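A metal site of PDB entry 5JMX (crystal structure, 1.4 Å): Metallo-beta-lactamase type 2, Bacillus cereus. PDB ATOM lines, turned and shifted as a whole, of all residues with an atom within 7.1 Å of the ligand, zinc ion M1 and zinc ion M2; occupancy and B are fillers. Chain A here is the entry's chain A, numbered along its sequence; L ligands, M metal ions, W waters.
Water W2 bridges O2 of the ligand and N of Asn 180.
Water W1 lies within hydrogen-bond range of the side-chain amino group (NZ) of Lys 171, the backbone carbonyl oxygen (O) of Cys 168 and an oxygen (O2) of the ligand.
Water W3 lies within hydrogen-bond range of the side-chain carboxylate of Asp 90 (2.8 Å) and the backbone NH of Ala 89 (3.4 Å).
Of the 26 residues printed, 4 come within 4 Å of zinc ion M2.
The side-chain sulfur of Cys 168 sits close to the guanidinium group of Arg 91, 3.6 Å away.
NE of Arg 91 lies within salt-bridge range of OD1 of Asp 90 (3.6 Å).
The backbone carbonyl oxygen of Pro 40 lies within hydrogen-bond range of a ring nitrogen (ND1) of His 210, at 2.7 Å.
OD1 of Asn 180 sits at hydrogen-bond distance from N of Ala 182 (2.8 Å).
O of Leu 178 sits at hydrogen-bond distance from NZ of Lys 171 (3.2 Å).
A ring nitrogen (NE2) of His 88 sits at hydrogen-bond distance from the side-chain carboxylate of Asp 183, at 2.6 Å.
Merely in contact with the ligand: Asn 180 (3.6 Å) and Asp 183 (3.7 Å).
Hydrophobic or aromatic side chains that line the ligand: His 88, His 149 and His 210.
NZ of Lys 171 lies within salt-bridge range of O2 of the ligand.
Zinc ion M1 is bound by a ring nitrogen (NE2) of His 210 (2.1 Å), the side-chain carboxylate (OD2) of Asp 90 (2.1 Å), an oxygen (O1) of the ligand (2.2 Å), the side-chain sulfur (SG) of Cys 168 (2.3 Å) and a sulfur (S1) of the ligand (2.4 Å).
Zinc ion M1 has five donor atoms within binding distance.
Three residues have an atom within 4 Å of zinc ion M1: Asp 90, Cys 168 and His 210.
The nearest printed residue that does not touch zinc ion M1 is Arg 91 (4.04 Å).
Zinc ion M2 is bound by NE2 of His 149.
A ring nitrogen (NE2) of His 86 binds zinc ion M2 (2.0 Å).
A ring nitrogen (ND1) of His 88 is bound to zinc ion M2, 2.1 Å away.
S1 of the ligand binds zinc ion M2, at 2.3 Å.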
ATOM      1  N   PRO A  40     -16.840 -27.401  14.225  1.00  0.00           N
ATOM      2  CA  PRO A  40     -16.121 -27.841  15.418  1.00  0.00           C
ATOM      3  C   PRO A  40     -17.061 -27.985  16.596  1.00  0.00           C
ATOM      4  O   PRO A  40     -18.085 -27.296  16.689  1.00  0.00           O
ATOM      5  CB  PRO A  40     -15.144 -26.692  15.670  1.00  0.00           C
ATOM      6  CG  PRO A  40     -15.862 -25.520  15.212  1.00  0.00           C
ATOM      7  CD  PRO A  40     -16.699 -25.957  14.027  1.00  0.00           C
ATOM      8  N   SER A  41     -16.676 -28.884  17.480  1.00  0.00           N
ATOM      9  CA  SER A  41     -17.414 -29.150  18.708  1.00  0.00           C
ATOM     10  C   SER A  41     -16.412 -29.310  19.842  1.00  0.00           C
ATOM     11  O   SER A  41     -15.330 -29.888  19.620  1.00  0.00           O
ATOM     12  CB  SER A  41     -18.203 -30.456  18.541  1.00  0.00           C
ATOM     13  OG  SER A  41     -18.668 -30.950  19.789  1.00  0.00           O
ATOM     14  N   TRP A  59     -18.583 -36.464  17.380  1.00  0.00           N
ATOM     15  CA  TRP A  59     -19.649 -36.583  16.395  1.00  0.00           C
ATOM     16  C   TRP A  59     -19.941 -38.028  16.008  1.00  0.00           C
ATOM     17  O   TRP A  59     -21.067 -38.346  15.634  1.00  0.00           O
ATOM     18  CB  TRP A  59     -19.201 -35.856  15.146  1.00  0.00           C
ATOM     19  CG  TRP A  59     -18.991 -34.385  15.312  1.00  0.00           C
ATOM     20  CD1 TRP A  59     -17.823 -33.733  15.577  1.00  0.00           C
ATOM     21  CD2 TRP A  59     -19.994 -33.368  15.185  1.00  0.00           C
ATOM     22  NE1 TRP A  59     -18.034 -32.364  15.602  1.00  0.00           N
ATOM     23  CE2 TRP A  59     -19.359 -32.121  15.376  1.00  0.00           C
ATOM     24  CE3 TRP A  59     -21.357 -33.398  14.944  1.00  0.00           C
ATOM     25  CZ2 TRP A  59     -20.054 -30.912  15.319  1.00  0.00           C
ATOM     26  CZ3 TRP A  59     -22.043 -32.194  14.888  1.00  0.00           C
ATOM     27  CH2 TRP A  59     -21.392 -30.979  15.086  1.00  0.00           C
ATOM     28  N   HIS A  86     -25.910 -33.892  26.439  1.00  0.00           N
ATOM     29  CA  HIS A  86     -27.241 -34.052  25.857  1.00  0.00           C
ATOM     30  C   HIS A  86     -27.162 -35.098  24.764  1.00  0.00           C
ATOM     31  O   HIS A  86     -26.099 -35.610  24.438  1.00  0.00           O
ATOM     32  CB  HIS A  86     -27.902 -32.736  25.406  1.00  0.00           C
ATOM     33  CG  HIS A  86     -27.303 -32.080  24.196  1.00  0.00           C
ATOM     34  ND1 HIS A  86     -26.211 -31.231  24.312  1.00  0.00           N
ATOM     35  CD2 HIS A  86     -27.735 -31.951  22.917  1.00  0.00           C
ATOM     36  CE1 HIS A  86     -25.931 -30.723  23.126  1.00  0.00           C
ATOM     37  NE2 HIS A  86     -26.828 -31.148  22.252  1.00  0.00           N
ATOM     38  N   ALA A  87     -28.318 -35.470  24.225  1.00  0.00           N
ATOM     39  CA  ALA A  87     -28.383 -36.602  23.315  1.00  0.00           C
ATOM     40  C   ALA A  87     -28.357 -36.224  21.837  1.00  0.00           C
ATOM     41  O   ALA A  87     -29.021 -36.859  21.018  1.00  0.00           O
ATOM     42  CB  ALA A  87     -29.651 -37.412  23.622  1.00  0.00           C
ATOM     43  N   HIS A  88     -27.576 -35.237  21.419  1.00  0.00           N
ATOM     44  CA  HIS A  88     -27.314 -34.998  20.015  1.00  0.00           C
ATOM     45  C   HIS A  88     -25.958 -35.599  19.635  1.00  0.00           C
ATOM     46  O   HIS A  88     -25.121 -35.856  20.485  1.00  0.00           O
ATOM     47  CB  HIS A  88     -27.279 -33.487  19.770  1.00  0.00           C
ATOM     48  CG  HIS A  88     -28.604 -32.828  19.664  1.00  0.00           C
ATOM     49  ND1 HIS A  88     -28.782 -31.467  19.834  1.00  0.00           N
ATOM     50  CD2 HIS A  88     -29.822 -33.320  19.328  1.00  0.00           C
ATOM     51  CE1 HIS A  88     -30.056 -31.168  19.640  1.00  0.00           C
ATOM     52  NE2 HIS A  88     -30.703 -32.267  19.301  1.00  0.00           N
ATOM     53  N   ALA A  89     -25.719 -35.765  18.322  1.00  0.00           N
ATOM     54  CA  ALA A  89     -24.584 -36.553  17.854  1.00  0.00           C
ATOM     55  C   ALA A  89     -23.254 -35.931  18.243  1.00  0.00           C
ATOM     56  O   ALA A  89     -22.293 -36.649  18.478  1.00  0.00           O
ATOM     57  CB  ALA A  89     -24.653 -36.699  16.333  1.00  0.00           C
ATOM     58  N   ASP A  90     -23.154 -34.600  18.297  1.00  0.00           N
ATOM     59  CA  ASP A  90     -21.880 -34.013  18.701  1.00  0.00           C
ATOM     60  C   ASP A  90     -21.478 -34.407  20.117  1.00  0.00           C
ATOM     61  O   ASP A  90     -20.283 -34.405  20.447  1.00  0.00           O
ATOM     62  CB  ASP A  90     -21.886 -32.484  18.492  1.00  0.00           C
ATOM     63  CG  ASP A  90     -22.891 -31.758  19.361  1.00  0.00           C
ATOM     64  OD1 ASP A  90     -23.961 -32.319  19.683  1.00  0.00           O
ATOM     65  OD2 ASP A  90     -22.657 -30.540  19.654  1.00  0.00           O
ATOM     66  N   ARG A  91     -22.432 -34.757  20.964  1.00  0.00           N
ATOM     67  CA  ARG A  91     -22.158 -35.140  22.343  1.00  0.00           C
ATOM     68  C   ARG A  91     -22.049 -36.646  22.491  1.00  0.00           C
ATOM     69  O   ARG A  91     -21.198 -37.125  23.248  1.00  0.00           O
ATOM     70  CB  ARG A  91     -23.296 -34.655  23.270  1.00  0.00           C
ATOM     71  CG  ARG A  91     -23.700 -33.195  23.140  1.00  0.00           C
ATOM     72  CD  ARG A  91     -22.605 -32.290  23.633  1.00  0.00           C
ATOM     73  NE  ARG A  91     -21.999 -31.549  22.550  1.00  0.00           N
ATOM     74  CZ  ARG A  91     -20.900 -30.809  22.665  1.00  0.00           C
ATOM     75  NH1 ARG A  91     -20.248 -30.749  23.808  1.00  0.00           N
ATOM     76  NH2 ARG A  91     -20.478 -30.115  21.635  1.00  0.00           N
ATOM     77  N   HIS A 149     -31.225 -25.403  24.869  1.00  0.00           N
ATOM     78  CA  HIS A 149     -30.857 -25.891  23.557  1.00  0.00           C
ATOM     79  C   HIS A 149     -31.554 -27.211  23.265  1.00  0.00           C
ATOM     80  O   HIS A 149     -31.971 -27.468  22.125  1.00  0.00           O
ATOM     81  CB  HIS A 149     -29.347 -26.091  23.549  1.00  0.00           C
ATOM     82  CG  HIS A 149     -28.861 -26.938  22.417  1.00  0.00           C
ATOM     83  ND1 HIS A 149     -28.926 -26.539  21.104  1.00  0.00           N
ATOM     84  CD2 HIS A 149     -28.357 -28.199  22.394  1.00  0.00           C
ATOM     85  CE1 HIS A 149     -28.448 -27.479  20.323  1.00  0.00           C
ATOM     86  NE2 HIS A 149     -28.096 -28.507  21.087  1.00  0.00           N
ATOM     87  N   THR A 150     -31.671 -28.063  24.284  1.00  0.00           N
ATOM     88  CA  THR A 150     -32.515 -29.235  24.234  1.00  0.00           C
ATOM     89  C   THR A 150     -33.243 -29.377  25.552  1.00  0.00           C
ATOM     90  O   THR A 150     -33.014 -28.638  26.518  1.00  0.00           O
ATOM     91  CB  THR A 150     -31.716 -30.513  24.013  1.00  0.00           C
ATOM     92  OG1 THR A 150     -30.785 -30.626  25.105  1.00  0.00           O
ATOM     93  CG2 THR A 150     -31.059 -30.521  22.668  1.00  0.00           C
ATOM     94  N   GLY A 167     -21.599 -26.441  27.386  1.00  0.00           N
ATOM     95  CA  GLY A 167     -22.160 -27.250  26.369  1.00  0.00           C
ATOM     96  C   GLY A 167     -22.975 -26.387  25.423  1.00  0.00           C
ATOM     97  O   GLY A 167     -22.756 -25.182  25.270  1.00  0.00           O
ATOM     98  N   CYS A 168     -23.926 -27.041  24.760  1.00  0.00           N
ATOM     99  CA  CYS A 168     -24.620 -26.363  23.689  1.00  0.00           C
ATOM    100  C   CYS A 168     -25.691 -25.432  24.195  1.00  0.00           C
ATOM    101  O   CYS A 168     -26.240 -24.656  23.396  1.00  0.00           O
ATOM    102  CB  CYS A 168     -25.085 -27.371  22.659  1.00  0.00           C
ATOM    103  SG  CYS A 168     -23.643 -28.380  22.080  1.00  0.00           S
ATOM    104  N   LEU A 169     -25.957 -25.435  25.516  1.00  0.00           N
ATOM    105  CA  LEU A 169     -26.749 -24.391  26.145  1.00  0.00           C
ATOM    106  C   LEU A 169     -26.113 -23.019  26.009  1.00  0.00           C
ATOM    107  O   LEU A 169     -26.829 -22.003  26.066  1.00  0.00           O
ATOM    108  CB  LEU A 169     -26.912 -24.723  27.630  1.00  0.00           C
ATOM    109  CG  LEU A 169     -27.799 -23.839  28.456  1.00  0.00           C
ATOM    110  CD1 LEU A 169     -29.246 -24.159  28.141  1.00  0.00           C
ATOM    111  CD2 LEU A 169     -27.489 -24.053  29.938  1.00  0.00           C
ATOM    112  N   VAL A 170     -24.799 -22.928  25.851  1.00  0.00           N
ATOM    113  CA  VAL A 170     -24.056 -21.678  25.863  1.00  0.00           C
ATOM    114  C   VAL A 170     -23.461 -21.480  24.479  1.00  0.00           C
ATOM    115  O   VAL A 170     -22.732 -22.338  23.978  1.00  0.00           O
ATOM    116  CB  VAL A 170     -22.972 -21.705  26.956  1.00  0.00           C
ATOM    117  CG1 VAL A 170     -22.175 -20.410  26.931  1.00  0.00           C
ATOM    118  CG2 VAL A 170     -23.596 -21.901  28.318  1.00  0.00           C
ATOM    119  N   LYS A 171     -23.751 -20.325  23.868  1.00  0.00           N
ATOM    120  CA  LYS A 171     -23.220 -19.970  22.576  1.00  0.00           C
ATOM    121  C   LYS A 171     -21.935 -19.183  22.721  1.00  0.00           C
ATOM    122  O   LYS A 171     -21.756 -18.398  23.646  1.00  0.00           O
ATOM    123  CB  LYS A 171     -24.237 -19.114  21.807  1.00  0.00           C
ATOM    124  CG  LYS A 171     -25.625 -19.702  21.724  1.00  0.00           C
ATOM    125  CD  LYS A 171     -25.709 -21.081  21.110  1.00  0.00           C
ATOM    126  CE  LYS A 171     -25.249 -21.149  19.687  1.00  0.00           C
ATOM    127  NZ  LYS A 171     -25.616 -22.513  19.080  1.00  0.00           N
ATOM    128  N   LEU A 178     -28.998 -18.625  17.380  1.00  0.00           N
ATOM    129  CA  LEU A 178     -29.053 -19.766  18.280  1.00  0.00           C
ATOM    130  C   LEU A 178     -28.736 -21.087  17.600  1.00  0.00           C
ATOM    131  O   LEU A 178     -28.680 -22.104  18.290  1.00  0.00           O
ATOM    132  CB  LEU A 178     -30.426 -19.839  18.941  1.00  0.00           C
ATOM    133  CG  LEU A 178     -30.761 -18.659  19.848  1.00  0.00           C
ATOM    134  CD1 LEU A 178     -32.255 -18.646  20.143  1.00  0.00           C
ATOM    135  CD2 LEU A 178     -29.937 -18.693  21.115  1.00  0.00           C
ATOM    136  N   GLY A 179     -28.552 -21.106  16.280  1.00  0.00           N
ATOM    137  CA  GLY A 179     -28.303 -22.364  15.596  1.00  0.00           C
ATOM    138  C   GLY A 179     -29.592 -23.135  15.388  1.00  0.00           C
ATOM    139  O   GLY A 179     -30.682 -22.564  15.306  1.00  0.00           O
ATOM    140  N   ASN A 180     -29.484 -24.454  15.299  1.00  0.00           N
ATOM    141  CA  ASN A 180     -30.663 -25.283  15.054  1.00  0.00           C
ATOM    142  C   ASN A 180     -31.479 -25.368  16.328  1.00  0.00           C
ATOM    143  O   ASN A 180     -30.973 -25.835  17.365  1.00  0.00           O
ATOM    144  CB  ASN A 180     -30.225 -26.669  14.573  1.00  0.00           C
ATOM    145  CG  ASN A 180     -31.393 -27.545  14.144  1.00  0.00           C
ATOM    146  OD1 ASN A 180     -32.443 -27.566  14.778  1.00  0.00           O
ATOM    147  ND2 ASN A 180     -31.227 -28.260  13.026  1.00  0.00           N
ATOM    148  N   VAL A 181     -32.715 -24.903  16.289  1.00  0.00           N
ATOM    149  CA  VAL A 181     -33.588 -24.830  17.452  1.00  0.00           C
ATOM    150  C   VAL A 181     -34.711 -25.868  17.368  1.00  0.00           C
ATOM    151  O   VAL A 181     -35.693 -25.784  18.107  1.00  0.00           O
ATOM    152  CB  VAL A 181     -34.120 -23.404  17.688  1.00  0.00           C
ATOM    153  CG1 VAL A 181     -32.974 -22.472  18.087  1.00  0.00           C
ATOM    154  CG2 VAL A 181     -34.876 -22.880  16.438  1.00  0.00           C
ATOM    155  N   ALA A 182     -34.563 -26.862  16.492  1.00  0.00           N
ATOM    156  CA  ALA A 182     -35.610 -27.854  16.301  1.00  0.00           C
ATOM    157  C   ALA A 182     -35.939 -28.560  17.612  1.00  0.00           C
ATOM    158  O   ALA A 182     -37.092 -28.891  17.889  1.00  0.00           O
ATOM    159  CB  ALA A 182     -35.178 -28.878  15.258  1.00  0.00           C
ATOM    160  N   ASP A 183     -34.926 -28.821  18.428  1.00  0.00           N
ATOM    161  CA  ASP A 183     -35.147 -29.492  19.696  1.00  0.00           C
ATOM    162  C   ASP A 183     -35.111 -28.547  20.883  1.00  0.00           C
ATOM    163  O   ASP A 183     -35.019 -29.023  22.027  1.00  0.00           O
ATOM    164  CB  ASP A 183     -34.112 -30.601  19.881  1.00  0.00           C
ATOM    165  CG  ASP A 183     -34.230 -31.675  18.836  1.00  0.00           C
ATOM    166  OD1 ASP A 183     -35.355 -31.944  18.332  1.00  0.00           O
ATOM    167  OD2 ASP A 183     -33.211 -32.324  18.523  1.00  0.00           O
ATOM    168  N   ALA A 184     -35.192 -27.232  20.668  1.00  0.00           N
ATOM    169  CA  ALA A 184     -34.939 -26.252  21.694  1.00  0.00           C
ATOM    170  C   ALA A 184     -36.235 -25.735  22.295  1.00  0.00           C
ATOM    171  O   ALA A 184     -37.330 -25.955  21.773  1.00  0.00           O
ATOM    172  CB  ALA A 184     -34.141 -25.091  21.114  1.00  0.00           C
ATOM    173  N   TRP A 189     -35.125 -21.298  27.785  1.00  0.00           N
ATOM    174  CA  TRP A 189     -33.657 -21.261  27.713  1.00  0.00           C
ATOM    175  C   TRP A 189     -33.088 -20.103  28.517  1.00  0.00           C
ATOM    176  O   TRP A 189     -32.061 -20.255  29.183  1.00  0.00           O
ATOM    177  CB  TRP A 189     -33.288 -21.179  26.230  1.00  0.00           C
ATOM    178  CG  TRP A 189     -31.881 -21.449  25.834  1.00  0.00           C
ATOM    179  CD1 TRP A 189     -30.727 -21.389  26.610  1.00  0.00           C
ATOM    180  CD2 TRP A 189     -31.460 -21.804  24.521  1.00  0.00           C
ATOM    181  NE1 TRP A 189     -29.636 -21.662  25.816  1.00  0.00           N
ATOM    182  CE2 TRP A 189     -30.058 -21.959  24.552  1.00  0.00           C
ATOM    183  CE3 TRP A 189     -32.143 -22.051  23.339  1.00  0.00           C
ATOM    184  CZ2 TRP A 189     -29.331 -22.306  23.401  1.00  0.00           C
ATOM    185  CZ3 TRP A 189     -31.443 -22.380  22.205  1.00  0.00           C
ATOM    186  CH2 TRP A 189     -30.032 -22.538  22.246  1.00  0.00           C
ATOM    187  N   GLY A 209     -20.356 -25.228  23.735  1.00  0.00           N
ATOM    188  CA  GLY A 209     -20.400 -26.433  22.960  1.00  0.00           C
ATOM    189  C   GLY A 209     -19.640 -26.333  21.651  1.00  0.00           C
ATOM    190  O   GLY A 209     -19.099 -27.335  21.168  1.00  0.00           O
ATOM    191  N   HIS A 210     -19.610 -25.144  21.047  1.00  0.00           N
ATOM    192  CA  HIS A 210     -18.924 -24.873  19.796  1.00  0.00           C
ATOM    193  C   HIS A 210     -18.312 -23.482  19.920  1.00  0.00           C
ATOM    194  O   HIS A 210     -18.983 -22.567  20.403  1.00  0.00           O
ATOM    195  CB  HIS A 210     -19.926 -24.910  18.605  1.00  0.00           C
ATOM    196  CG  HIS A 210     -20.803 -26.125  18.613  1.00  0.00           C
ATOM    197  ND1 HIS A 210     -20.460 -27.295  17.948  1.00  0.00           N
ATOM    198  CD2 HIS A 210     -21.954 -26.398  19.277  1.00  0.00           C
ATOM    199  CE1 HIS A 210     -21.393 -28.209  18.174  1.00  0.00           C
ATOM    200  NE2 HIS A 210     -22.297 -27.703  18.995  1.00  0.00           N
HETATM  201  O1  LIG L   1     -25.015 -26.961  19.491  1.00  0.00           O
HETATM  202  C1  LIG L   1     -25.781 -27.026  18.487  1.00  0.00           C
HETATM  203  O2  LIG L   1     -26.172 -25.987  17.882  1.00  0.00           O
HETATM  204  C2  LIG L   1     -26.391 -28.377  18.102  1.00  0.00           C
HETATM  205  C3  LIG L   1     -27.454 -28.421  17.235  1.00  0.00           C
HETATM  206  C4  LIG L   1     -28.254 -29.581  16.829  1.00  0.00           C
HETATM  207  C5  LIG L   1     -27.768 -30.842  16.430  1.00  0.00           C
HETATM  208  C6  LIG L   1     -28.604 -31.893  16.065  1.00  0.00           C
HETATM  209  C7  LIG L   1     -29.986 -31.648  16.090  1.00  0.00           C
HETATM  210  F1  LIG L   1     -30.844 -32.671  15.739  1.00  0.00           F
HETATM  211  C8  LIG L   1     -30.543 -30.478  16.462  1.00  0.00           C
HETATM  212  C9  LIG L   1     -29.672 -29.449  16.822  1.00  0.00           C
HETATM  213  S1  LIG L   1     -25.732 -29.817  18.808  1.00  0.00           S
HETATM  214 ZN    ZN M   1     -23.859 -28.792  19.858  1.00  0.00          ZN
HETATM  215 ZN    ZN M   2     -27.267 -30.237  20.469  1.00  0.00          ZN
HETATM  216  O   HOH W   1     -24.950 -24.551  20.796  1.00  0.00           O
HETATM  217  O   HOH W   2     -26.971 -25.592  15.323  1.00  0.00           O
HETATM  218  O   HOH W   3     -24.958 -32.668  17.084  1.00  0.00           O
